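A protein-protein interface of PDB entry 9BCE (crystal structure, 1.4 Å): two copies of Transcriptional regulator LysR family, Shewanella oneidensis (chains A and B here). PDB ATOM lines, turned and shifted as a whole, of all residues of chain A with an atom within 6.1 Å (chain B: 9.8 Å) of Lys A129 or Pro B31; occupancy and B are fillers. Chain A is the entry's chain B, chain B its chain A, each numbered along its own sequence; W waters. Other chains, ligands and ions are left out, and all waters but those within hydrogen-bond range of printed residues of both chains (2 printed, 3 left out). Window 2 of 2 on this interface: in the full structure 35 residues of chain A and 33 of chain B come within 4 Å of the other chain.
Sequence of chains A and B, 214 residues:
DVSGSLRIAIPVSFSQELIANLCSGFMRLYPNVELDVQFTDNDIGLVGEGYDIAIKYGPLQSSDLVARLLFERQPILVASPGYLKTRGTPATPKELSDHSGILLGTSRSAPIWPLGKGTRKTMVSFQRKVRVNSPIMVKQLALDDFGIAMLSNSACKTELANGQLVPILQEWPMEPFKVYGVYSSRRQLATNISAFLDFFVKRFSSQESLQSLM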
ATOM      1  N   SER A 100     -20.827   2.483  18.293  1.00  0.00           N
ATOM      2  CA  SER A 100     -19.648   2.807  17.496  1.00  0.00           C
ATOM      3  C   SER A 100     -19.522   4.315  17.339  1.00  0.00           C
ATOM      4  O   SER A 100     -20.480   4.992  16.943  1.00  0.00           O
ATOM      5  CB  SER A 100     -19.780   2.204  16.101  1.00  0.00           C
ATOM      6  OG  SER A 100     -19.817   0.803  16.166  1.00  0.00           O
ATOM      7  N   GLY A 101     -18.339   4.836  17.634  1.00  0.00           N
ATOM      8  CA  GLY A 101     -18.026   6.233  17.387  1.00  0.00           C
ATOM      9  C   GLY A 101     -16.890   6.404  16.395  1.00  0.00           C
ATOM     10  O   GLY A 101     -16.031   5.536  16.254  1.00  0.00           O
ATOM     11  N   ILE A 102     -16.909   7.539  15.699  1.00  0.00           N
ATOM     12  CA  ILE A 102     -15.889   7.945  14.739  1.00  0.00           C
ATOM     13  C   ILE A 102     -15.144   9.099  15.396  1.00  0.00           C
ATOM     14  O   ILE A 102     -15.689  10.211  15.490  1.00  0.00           O
ATOM     15  CB  ILE A 102     -16.513   8.370  13.404  1.00  0.00           C
ATOM     16  CG1 ILE A 102     -17.347   7.227  12.810  1.00  0.00           C
ATOM     17  CG2 ILE A 102     -15.430   8.843  12.411  1.00  0.00           C
ATOM     18  CD1 ILE A 102     -18.444   7.685  11.861  1.00  0.00           C
ATOM     19  N   PHE A 126     -16.876   5.461  24.045  1.00  0.00           N
ATOM     20  CA  PHE A 126     -17.620   4.790  22.992  1.00  0.00           C
ATOM     21  C   PHE A 126     -16.650   3.798  22.367  1.00  0.00           C
ATOM     22  O   PHE A 126     -15.440   3.839  22.630  1.00  0.00           O
ATOM     23  CB  PHE A 126     -18.132   5.795  21.947  1.00  0.00           C
ATOM     24  CG  PHE A 126     -17.058   6.718  21.401  1.00  0.00           C
ATOM     25  CD1 PHE A 126     -16.270   6.326  20.331  1.00  0.00           C
ATOM     26  CD2 PHE A 126     -16.828   7.966  21.977  1.00  0.00           C
ATOM     27  CE1 PHE A 126     -15.294   7.168  19.812  1.00  0.00           C
ATOM     28  CE2 PHE A 126     -15.841   8.812  21.479  1.00  0.00           C
ATOM     29  CZ  PHE A 126     -15.073   8.415  20.389  1.00  0.00           C
ATOM     30  N   GLN A 127     -17.191   2.899  21.546  1.00  0.00           N
ATOM     31  CA  GLN A 127     -16.356   1.938  20.835  1.00  0.00           C
ATOM     32  C   GLN A 127     -15.655   2.665  19.697  1.00  0.00           C
ATOM     33  O   GLN A 127     -16.313   3.234  18.822  1.00  0.00           O
ATOM     34  CB  GLN A 127     -17.215   0.800  20.289  1.00  0.00           C
ATOM     35  CG  GLN A 127     -17.922  -0.023  21.350  1.00  0.00           C
ATOM     36  CD  GLN A 127     -19.094  -0.802  20.772  1.00  0.00           C
ATOM     37  OE1 GLN A 127     -19.249  -0.896  19.558  1.00  0.00           O
ATOM     38  NE2 GLN A 127     -19.919  -1.366  21.644  1.00  0.00           N
ATOM     39  N   ARG A 128     -14.325   2.639  19.690  1.00  0.00           N
ATOM     40  CA  ARG A 128     -13.554   3.440  18.730  1.00  0.00           C
ATOM     41  C   ARG A 128     -13.416   2.700  17.400  1.00  0.00           C
ATOM     42  O   ARG A 128     -12.382   2.098  17.087  1.00  0.00           O
ATOM     43  CB  ARG A 128     -12.188   3.808  19.293  1.00  0.00           C
ATOM     44  CG  ARG A 128     -11.491   4.915  18.521  1.00  0.00           C
ATOM     45  CD  ARG A 128     -10.020   4.982  18.875  1.00  0.00           C
ATOM     46  NE  ARG A 128      -9.236   4.053  18.067  1.00  0.00           N
ATOM     47  CZ  ARG A 128      -7.925   3.891  18.176  1.00  0.00           C
ATOM     48  NH1 ARG A 128      -7.208   4.597  19.037  1.00  0.00           N
ATOM     49  NH2 ARG A 128      -7.314   2.999  17.404  1.00  0.00           N
ATOM     50  N   LYS A 129     -14.479   2.777  16.591  1.00  0.00           N
ATOM     51  CA  LYS A 129     -14.496   2.095  15.296  1.00  0.00           C
ATOM     52  C   LYS A 129     -13.438   2.664  14.355  1.00  0.00           C
ATOM     53  O   LYS A 129     -12.739   1.912  13.650  1.00  0.00           O
ATOM     54  CB  LYS A 129     -15.895   2.202  14.683  1.00  0.00           C
ATOM     55  CG  LYS A 129     -16.023   1.558  13.320  1.00  0.00           C
ATOM     56  CD  LYS A 129     -15.954   0.034  13.394  1.00  0.00           C
ATOM     57  CE  LYS A 129     -16.147  -0.613  12.008  1.00  0.00           C
ATOM     58  NZ  LYS A 129     -16.132  -2.103  12.062  1.00  0.00           N
ATOM     59  N   VAL A 130     -13.307   3.989  14.327  1.00  0.00           N
ATOM     60  CA  VAL A 130     -12.297   4.682  13.533  1.00  0.00           C
ATOM     61  C   VAL A 130     -11.736   5.808  14.384  1.00  0.00           C
ATOM     62  O   VAL A 130     -12.477   6.472  15.120  1.00  0.00           O
ATOM     63  CB  VAL A 130     -12.902   5.293  12.249  1.00  0.00           C
ATOM     64  CG1 VAL A 130     -11.878   6.182  11.523  1.00  0.00           C
ATOM     65  CG2 VAL A 130     -13.402   4.206  11.321  1.00  0.00           C
ATOM     66  N   ARG A 131     -10.427   6.014  14.301  1.00  0.00           N
ATOM     67  CA  ARG A 131      -9.806   7.271  14.691  1.00  0.00           C
ATOM     68  C   ARG A 131      -9.133   7.843  13.449  1.00  0.00           C
ATOM     69  O   ARG A 131      -8.455   7.115  12.718  1.00  0.00           O
ATOM     70  CB  ARG A 131      -8.764   7.072  15.793  1.00  0.00           C
ATOM     71  CG  ARG A 131      -8.074   8.396  16.175  1.00  0.00           C
ATOM     72  CD  ARG A 131      -7.209   8.288  17.425  1.00  0.00           C
ATOM     73  NE  ARG A 131      -6.052   7.423  17.235  1.00  0.00           N
ATOM     74  CZ  ARG A 131      -5.210   7.099  18.203  1.00  0.00           C
ATOM     75  NH1 ARG A 131      -5.400   7.519  19.446  1.00  0.00           N
ATOM     76  NH2 ARG A 131      -4.165   6.316  17.924  1.00  0.00           N
ATOM     77  N   PHE A 146     -21.381   4.292   9.653  1.00  0.00           N
ATOM     78  CA  PHE A 146     -20.400   3.639  10.502  1.00  0.00           C
ATOM     79  C   PHE A 146     -20.538   3.983  11.970  1.00  0.00           C
ATOM     80  O   PHE A 146     -19.952   3.278  12.805  1.00  0.00           O
ATOM     81  CB  PHE A 146     -18.979   3.917  10.014  1.00  0.00           C
ATOM     82  CG  PHE A 146     -18.588   3.074   8.847  1.00  0.00           C
ATOM     83  CD1 PHE A 146     -18.339   1.719   9.011  1.00  0.00           C
ATOM     84  CD2 PHE A 146     -18.532   3.614   7.574  1.00  0.00           C
ATOM     85  CE1 PHE A 146     -17.999   0.934   7.927  1.00  0.00           C
ATOM     86  CE2 PHE A 146     -18.176   2.833   6.491  1.00  0.00           C
ATOM     87  CZ  PHE A 146     -17.918   1.494   6.672  1.00  0.00           C
ATOM     88  N   ASP B   1      -8.567 -14.867   8.369  1.00  0.00           N
ATOM     89  CA  ASP B   1      -9.560 -13.879   8.774  1.00  0.00           C
ATOM     90  C   ASP B   1      -8.959 -12.485   8.784  1.00  0.00           C
ATOM     91  O   ASP B   1      -7.856 -12.283   9.283  1.00  0.00           O
ATOM     92  CB  ASP B   1     -10.111 -14.204  10.161  1.00  0.00           C
ATOM     93  CG  ASP B   1     -11.552 -13.761  10.335  1.00  0.00           C
ATOM     94  OD1 ASP B   1     -12.445 -14.339   9.676  1.00  0.00           O
ATOM     95  OD2 ASP B   1     -11.791 -12.827  11.129  1.00  0.00           O
ATOM     96  N   VAL B   2      -9.692 -11.524   8.234  1.00  0.00           N
ATOM     97  CA  VAL B   2      -9.294 -10.123   8.253  1.00  0.00           C
ATOM     98  C   VAL B   2     -10.066  -9.461   9.387  1.00  0.00           C
ATOM     99  O   VAL B   2     -11.283  -9.273   9.295  1.00  0.00           O
ATOM    100  CB  VAL B   2      -9.563  -9.445   6.903  1.00  0.00           C
ATOM    101  CG1 VAL B   2      -9.232  -7.965   6.969  1.00  0.00           C
ATOM    102  CG2 VAL B   2      -8.754 -10.128   5.796  1.00  0.00           C
ATOM    103  N   SER B   3      -9.371  -9.121  10.469  1.00  0.00           N
ATOM    104  CA  SER B   3     -10.039  -8.581  11.646  1.00  0.00           C
ATOM    105  C   SER B   3      -8.995  -7.923  12.533  1.00  0.00           C
ATOM    106  O   SER B   3      -7.791  -8.137  12.376  1.00  0.00           O
ATOM    107  CB  SER B   3     -10.769  -9.680  12.419  1.00  0.00           C
ATOM    108  OG  SER B   3      -9.833 -10.607  12.931  1.00  0.00           O
ATOM    109  N   GLY B   4      -9.477  -7.123  13.476  1.00  0.00           N
ATOM    110  CA  GLY B   4      -8.600  -6.468  14.422  1.00  0.00           C
ATOM    111  C   GLY B   4      -8.371  -5.022  14.043  1.00  0.00           C
ATOM    112  O   GLY B   4      -9.275  -4.364  13.523  1.00  0.00           O
ATOM    113  N   SER B   5      -7.171  -4.510  14.272  1.00  0.00           N
ATOM    114  CA  SER B   5      -6.881  -3.100  14.060  1.00  0.00           C
ATOM    115  C   SER B   5      -5.836  -2.923  12.969  1.00  0.00           C
ATOM    116  O   SER B   5      -4.961  -3.766  12.779  1.00  0.00           O
ATOM    117  CB  SER B   5      -6.325  -2.489  15.330  1.00  0.00           C
ATOM    118  OG  SER B   5      -5.136  -3.160  15.694  1.00  0.00           O
ATOM    119  N   LEU B   6      -5.977  -1.850  12.192  1.00  0.00           N
ATOM    120  CA  LEU B   6      -4.941  -1.430  11.259  1.00  0.00           C
ATOM    121  C   LEU B   6      -4.665   0.032  11.539  1.00  0.00           C
ATOM    122  O   LEU B   6      -5.606   0.821  11.656  1.00  0.00           O
ATOM    123  CB  LEU B   6      -5.384  -1.576   9.797  1.00  0.00           C
ATOM    124  CG  LEU B   6      -5.088  -2.851   9.004  1.00  0.00           C
ATOM    125  CD1 LEU B   6      -5.612  -2.678   7.594  1.00  0.00           C
ATOM    126  CD2 LEU B   6      -3.602  -3.231   8.978  1.00  0.00           C
ATOM    127  N   ARG B   7      -3.389   0.382  11.656  1.00  0.00           N
ATOM    128  CA  ARG B   7      -2.934   1.756  11.817  1.00  0.00           C
ATOM    129  C   ARG B   7      -2.174   2.161  10.561  1.00  0.00           C
ATOM    130  O   ARG B   7      -1.220   1.477  10.164  1.00  0.00           O
ATOM    131  CB  ARG B   7      -1.965   1.834  12.993  1.00  0.00           C
ATOM    132  CG  ARG B   7      -2.530   1.422  14.328  1.00  0.00           C
ATOM    133  CD  ARG B   7      -1.665   2.015  15.441  1.00  0.00           C
ATOM    134  NE  ARG B   7      -1.767   3.471  15.441  1.00  0.00           N
ATOM    135  CZ  ARG B   7      -0.764   4.316  15.653  1.00  0.00           C
ATOM    136  NH1 ARG B   7       0.471   3.887  15.857  1.00  0.00           N
ATOM    137  NH2 ARG B   7      -1.008   5.629  15.662  1.00  0.00           N
ATOM    138  N   CYS B  23     -11.405   3.738   2.563  1.00  0.00           N
ATOM    139  CA  CYS B  23     -11.557   3.159   3.893  1.00  0.00           C
ATOM    140  C   CYS B  23     -12.995   2.737   4.154  1.00  0.00           C
ATOM    141  O   CYS B  23     -13.236   1.710   4.795  1.00  0.00           O
ATOM    142  CB  CYS B  23     -11.099   4.139   4.972  1.00  0.00           C
ATOM    143  SG  CYS B  23      -9.270   4.273   5.017  1.00  0.00           S
ATOM    144  N   SER B  24     -13.960   3.522   3.675  1.00  0.00           N
ATOM    145  CA  SER B  24     -15.352   3.117   3.779  1.00  0.00           C
ATOM    146  C   SER B  24     -15.571   1.790   3.056  1.00  0.00           C
ATOM    147  O   SER B  24     -16.168   0.859   3.607  1.00  0.00           O
ATOM    148  CB  SER B  24     -16.248   4.214   3.198  1.00  0.00           C
ATOM    149  OG  SER B  24     -17.608   3.797   3.195  1.00  0.00           O
ATOM    150  N   GLY B  25     -15.074   1.676   1.819  1.00  0.00           N
ATOM    151  CA  GLY B  25     -15.248   0.427   1.088  1.00  0.00           C
ATOM    152  C   GLY B  25     -14.568  -0.736   1.781  1.00  0.00           C
ATOM    153  O   GLY B  25     -15.124  -1.838   1.864  1.00  0.00           O
ATOM    154  N   PHE B  26     -13.370  -0.496   2.321  1.00  0.00           N
ATOM    155  CA  PHE B  26     -12.633  -1.552   2.998  1.00  0.00           C
ATOM    156  C   PHE B  26     -13.393  -2.064   4.213  1.00  0.00           C
ATOM    157  O   PHE B  26     -13.513  -3.276   4.421  1.00  0.00           O
ATOM    158  CB  PHE B  26     -11.259  -1.026   3.404  1.00  0.00           C
ATOM    159  CG  PHE B  26     -10.427  -2.034   4.110  1.00  0.00           C
ATOM    160  CD1 PHE B  26      -9.785  -3.045   3.399  1.00  0.00           C
ATOM    161  CD2 PHE B  26     -10.253  -1.968   5.478  1.00  0.00           C
ATOM    162  CE1 PHE B  26      -9.011  -3.971   4.052  1.00  0.00           C
ATOM    163  CE2 PHE B  26      -9.486  -2.906   6.135  1.00  0.00           C
ATOM    164  CZ  PHE B  26      -8.867  -3.910   5.425  1.00  0.00           C
ATOM    165  N   MET B  27     -13.927  -1.157   5.024  1.00  0.00           N
ATOM    166  CA  MET B  27     -14.620  -1.588   6.248  1.00  0.00           C
ATOM    167  C   MET B  27     -15.985  -2.215   5.962  1.00  0.00           C
ATOM    168  O   MET B  27     -16.482  -3.009   6.777  1.00  0.00           O
ATOM    169  CB  MET B  27     -14.763  -0.396   7.173  1.00  0.00           C
ATOM    170  CG  MET B  27     -13.450  -0.118   7.950  1.00  0.00           C
ATOM    171  SD  MET B  27     -13.635   1.119   9.386  1.00  0.00           S
ATOM    172  CE  MET B  27     -14.134   2.546   8.204  1.00  0.00           C
ATOM    173  N   ARG B  28     -16.599  -1.858   4.823  1.00  0.00           N
ATOM    174  CA  ARG B  28     -17.828  -2.536   4.420  1.00  0.00           C
ATOM    175  C   ARG B  28     -17.548  -3.958   3.946  1.00  0.00           C
ATOM    176  O   ARG B  28     -18.376  -4.851   4.147  1.00  0.00           O
ATOM    177  CB  ARG B  28     -18.544  -1.728   3.324  1.00  0.00           C
ATOM    178  CG  ARG B  28     -19.409  -0.593   3.865  1.00  0.00           C
ATOM    179  CD  ARG B  28     -19.711   0.473   2.816  1.00  0.00           C
ATOM    180  NE  ARG B  28     -20.728   1.411   3.278  1.00  0.00           N
ATOM    181  CZ  ARG B  28     -21.303   2.338   2.521  1.00  0.00           C
ATOM    182  NH1 ARG B  28     -20.963   2.503   1.251  1.00  0.00           N
ATOM    183  NH2 ARG B  28     -22.245   3.118   3.050  1.00  0.00           N
ATOM    184  N   LEU B  29     -16.384  -4.190   3.336  1.00  0.00           N
ATOM    185  CA  LEU B  29     -15.997  -5.540   2.939  1.00  0.00           C
ATOM    186  C   LEU B  29     -15.546  -6.359   4.143  1.00  0.00           C
ATOM    187  O   LEU B  29     -15.827  -7.563   4.226  1.00  0.00           O
ATOM    188  CB  LEU B  29     -14.882  -5.460   1.895  1.00  0.00           C
ATOM    189  CG  LEU B  29     -14.327  -6.788   1.392  1.00  0.00           C
ATOM    190  CD1 LEU B  29     -15.433  -7.630   0.777  1.00  0.00           C
ATOM    191  CD2 LEU B  29     -13.225  -6.528   0.379  1.00  0.00           C
ATOM    192  N   TYR B  30     -14.882  -5.704   5.098  1.00  0.00           N
ATOM    193  CA  TYR B  30     -14.278  -6.355   6.257  1.00  0.00           C
ATOM    194  C   TYR B  30     -14.822  -5.675   7.505  1.00  0.00           C
ATOM    195  O   TYR B  30     -14.150  -4.820   8.098  1.00  0.00           O
ATOM    196  CB  TYR B  30     -12.754  -6.249   6.196  1.00  0.00           C
ATOM    197  CG  TYR B  30     -12.138  -6.909   4.978  1.00  0.00           C
ATOM    198  CD1 TYR B  30     -12.199  -8.286   4.805  1.00  0.00           C
ATOM    199  CD2 TYR B  30     -11.469  -6.158   4.026  1.00  0.00           C
ATOM    200  CE1 TYR B  30     -11.626  -8.898   3.702  1.00  0.00           C
ATOM    201  CE2 TYR B  30     -10.882  -6.756   2.917  1.00  0.00           C
ATOM    202  CZ  TYR B  30     -10.951  -8.127   2.765  1.00  0.00           C
ATOM    203  OH  TYR B  30     -10.380  -8.719   1.660  1.00  0.00           O
ATOM    204  N   PRO B  31     -16.016  -6.069   7.964  1.00  0.00           N
ATOM    205  CA  PRO B  31     -16.677  -5.343   9.059  1.00  0.00           C
ATOM    206  C   PRO B  31     -16.049  -5.528  10.431  1.00  0.00           C
ATOM    207  O   PRO B  31     -16.497  -4.873  11.378  1.00  0.00           O
ATOM    208  CB  PRO B  31     -18.119  -5.882   9.022  1.00  0.00           C
ATOM    209  CG  PRO B  31     -18.005  -7.209   8.388  1.00  0.00           C
ATOM    210  CD  PRO B  31     -16.886  -7.111   7.388  1.00  0.00           C
ATOM    211  N   ASN B  32     -15.014  -6.355  10.581  1.00  0.00           N
ATOM    212  CA  ASN B  32     -14.383  -6.553  11.882  1.00  0.00           C
ATOM    213  C   ASN B  32     -13.028  -5.871  12.007  1.00  0.00           C
ATOM    214  O   ASN B  32     -12.242  -6.233  12.883  1.00  0.00           O
ATOM    215  CB  ASN B  32     -14.268  -8.037  12.205  1.00  0.00           C
ATOM    216  CG  ASN B  32     -15.609  -8.661  12.445  1.00  0.00           C
ATOM    217  OD1 ASN B  32     -16.418  -8.138  13.229  1.00  0.00           O
ATOM    218  ND2 ASN B  32     -15.881  -9.777  11.758  1.00  0.00           N
ATOM    219  N   VAL B  33     -12.727  -4.896  11.156  1.00  0.00           N
ATOM    220  CA  VAL B  33     -11.465  -4.165  11.235  1.00  0.00           C
ATOM    221  C   VAL B  33     -11.734  -2.766  11.770  1.00  0.00           C
ATOM    222  O   VAL B  33     -12.629  -2.067  11.280  1.00  0.00           O
ATOM    223  CB  VAL B  33     -10.719  -4.114   9.886  1.00  0.00           C
ATOM    224  CG1 VAL B  33      -9.348  -3.483  10.075  1.00  0.00           C
ATOM    225  CG2 VAL B  33     -10.525  -5.494   9.329  1.00  0.00           C
ATOM    226  N   GLU B  34     -10.935  -2.348  12.748  1.00  0.00           N
ATOM    227  CA  GLU B  34     -10.967  -0.987  13.279  1.00  0.00           C
ATOM    228  C   GLU B  34      -9.778  -0.236  12.693  1.00  0.00           C
ATOM    229  O   GLU B  34      -8.664  -0.762  12.682  1.00  0.00           O
ATOM    230  CB  GLU B  34     -10.815  -1.077  14.798  1.00  0.00           C
ATOM    231  CG  GLU B  34     -12.088  -1.519  15.535  1.00  0.00           C
ATOM    232  CD  GLU B  34     -12.037  -1.217  17.023  1.00  0.00           C
ATOM    233  OE1 GLU B  34     -13.120  -1.127  17.646  1.00  0.00           O
ATOM    234  OE2 GLU B  34     -10.927  -1.043  17.574  1.00  0.00           O
ATOM    235  N   LEU B  35     -10.005   0.969  12.189  1.00  0.00           N
ATOM    236  CA  LEU B  35      -8.951   1.733  11.529  1.00  0.00           C
ATOM    237  C   LEU B  35      -8.471   2.889  12.405  1.00  0.00           C
ATOM    238  O   LEU B  35      -9.263   3.533  13.102  1.00  0.00           O
ATOM    239  CB  LEU B  35      -9.427   2.302  10.190  1.00  0.00           C
ATOM    240  CG  LEU B  35      -9.743   1.294   9.088  1.00  0.00           C
ATOM    241  CD1 LEU B  35     -10.198   2.031   7.844  1.00  0.00           C
ATOM    242  CD2 LEU B  35      -8.524   0.430   8.802  1.00  0.00           C
ATOM    243  N   ASP B  36      -7.175   3.165  12.334  1.00  0.00           N
ATOM    244  CA  ASP B  36      -6.566   4.365  12.900  1.00  0.00           C
ATOM    245  C   ASP B  36      -5.752   4.962  11.768  1.00  0.00           C
ATOM    246  O   ASP B  36      -4.752   4.369  11.349  1.00  0.00           O
ATOM    247  CB  ASP B  36      -5.675   3.994  14.087  1.00  0.00           C
ATOM    248  CG  ASP B  36      -5.002   5.191  14.727  1.00  0.00           C
ATOM    249  OD1 ASP B  36      -5.484   6.343  14.557  1.00  0.00           O
ATOM    250  OD2 ASP B  36      -3.983   4.971  15.430  1.00  0.00           O
ATOM    251  N   VAL B  37      -6.210   6.086  11.219  1.00  0.00           N
ATOM    252  CA  VAL B  37      -5.599   6.699  10.042  1.00  0.00           C
ATOM    253  C   VAL B  37      -5.107   8.087  10.420  1.00  0.00           C
ATOM    254  O   VAL B  37      -5.888   8.923  10.898  1.00  0.00           O
ATOM    255  CB  VAL B  37      -6.588   6.761   8.865  1.00  0.00           C
ATOM    256  CG1 VAL B  37      -5.979   7.485   7.664  1.00  0.00           C
ATOM    257  CG2 VAL B  37      -7.033   5.358   8.475  1.00  0.00           C
HETATM  258  O   HOH W   1      -7.131   0.762  15.072  1.00  0.00           O
HETATM  259  O   HOH W   2      -4.499   2.679  17.200  1.00  0.00           O
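The backbone carbonyl oxygen (O) of Gly B4 sits at hydrogen-bond distance from the backbone NH (N) of Glu B34 (2.7 Å).
The backbone NH (N) of Leu B6 sits at hydrogen-bond distance from the backbone carbonyl oxygen (O) of Glu B34.
The backbone NH (N) of Asp B36 sits at hydrogen-bond distance from the backbone carbonyl oxygen (O) of Leu B6 (2.9 Å).
OD2 of Asp B36 lies within salt-bridge range of NE of Arg B7, 2.7 Å away.
The backbone carbonyl oxygen (O) of Gly A101 is in hydrogen-bond range of the backbone NH (N) of Lys A129.
No position is printed for both chains.
Hydrophobic or aromatic side chains of chain B that line the printed part of chain A: Met B27.
Among the printed residues, 15 pairs touch across the chains.
Among the printed residues, pairs that only touch across the chains: Val A130 with Leu B35 (3.3 Å), Lys A129 with Glu B34 (3.4 Å), Phe A146 with Ser B24 (3.5 Å), Phe A146 with Met B27 (3.6 Å), Lys A129 with Val B33 (3.6 Å), Val A130 with Met B27 (3.6 Å), Phe A146 with Arg B28 (3.8 Å), Arg A128 with Asp B36 (3.8 Å) and Arg A131 with Arg B7 (3.9 Å).
Water W2 lies within hydrogen-bond range of NH2 of Arg A128, OD2 of Asp B36 and NE of Arg B7.
Water W1 lies within hydrogen-bond range of the backbone carbonyl oxygen of Glu B34 (3.2 Å) and the guanidinium group of Arg A128 (3.2 Å).
Of chain B, only Pro B31 (2.9 Å), Val B33 (3.6 Å), Glu B34 (3.4 Å) and Leu B35 (3.2 Å) come within 4 Å of Lys A129.
Of the printed residues of chain B, Val A130 touches Met B27 (3.6 Å) and Leu B35 (3.3 Å).
Of the printed residues of chain B, Arg A131 touches Arg B7 (3.9 Å), Leu B35 (3.0 Å), Asp B36 (2.8 Å) and Val B37 (2.9 Å).
Printed residues of chain A within 4 Å of Arg B28: Phe A146 (3.8 Å).
Printed residues of chain A within 4 Å of Val B37: Arg A131 (2.9 Å).
The nearest residue of chain B that does not touch Lys A129 is Met B27 (4.02 Å).
The nearest printed residue of chain A that does not touch Val B37 is Val A130 (5.7 Å).
The backbone carbonyl oxygen (O) of Pro B31 lies within hydrogen-bond range of the side-chain amino group (NZ) of Lys A129 (2.9 Å).
The backbone NH (N) of Leu B35 lies within hydrogen-bond range of the backbone carbonyl oxygen (O) of Lys A129 (3.2 Å).
The backbone carbonyl oxygen (O) of Leu B35 is in hydrogen-bond range of the backbone NH (N) of Arg A131, 3.0 Å away.
OD2 of Asp B36 lies within salt-bridge range of NH2 of Arg A131 (2.8 Å).
O of Arg A131 sits at hydrogen-bond distance from N of Val B37 (2.9 Å).
The side-chain carboxylate (OE1) of Glu B34 lies close to the backbone carbonyl oxygen (O) of Arg A128 (3.4 Å).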
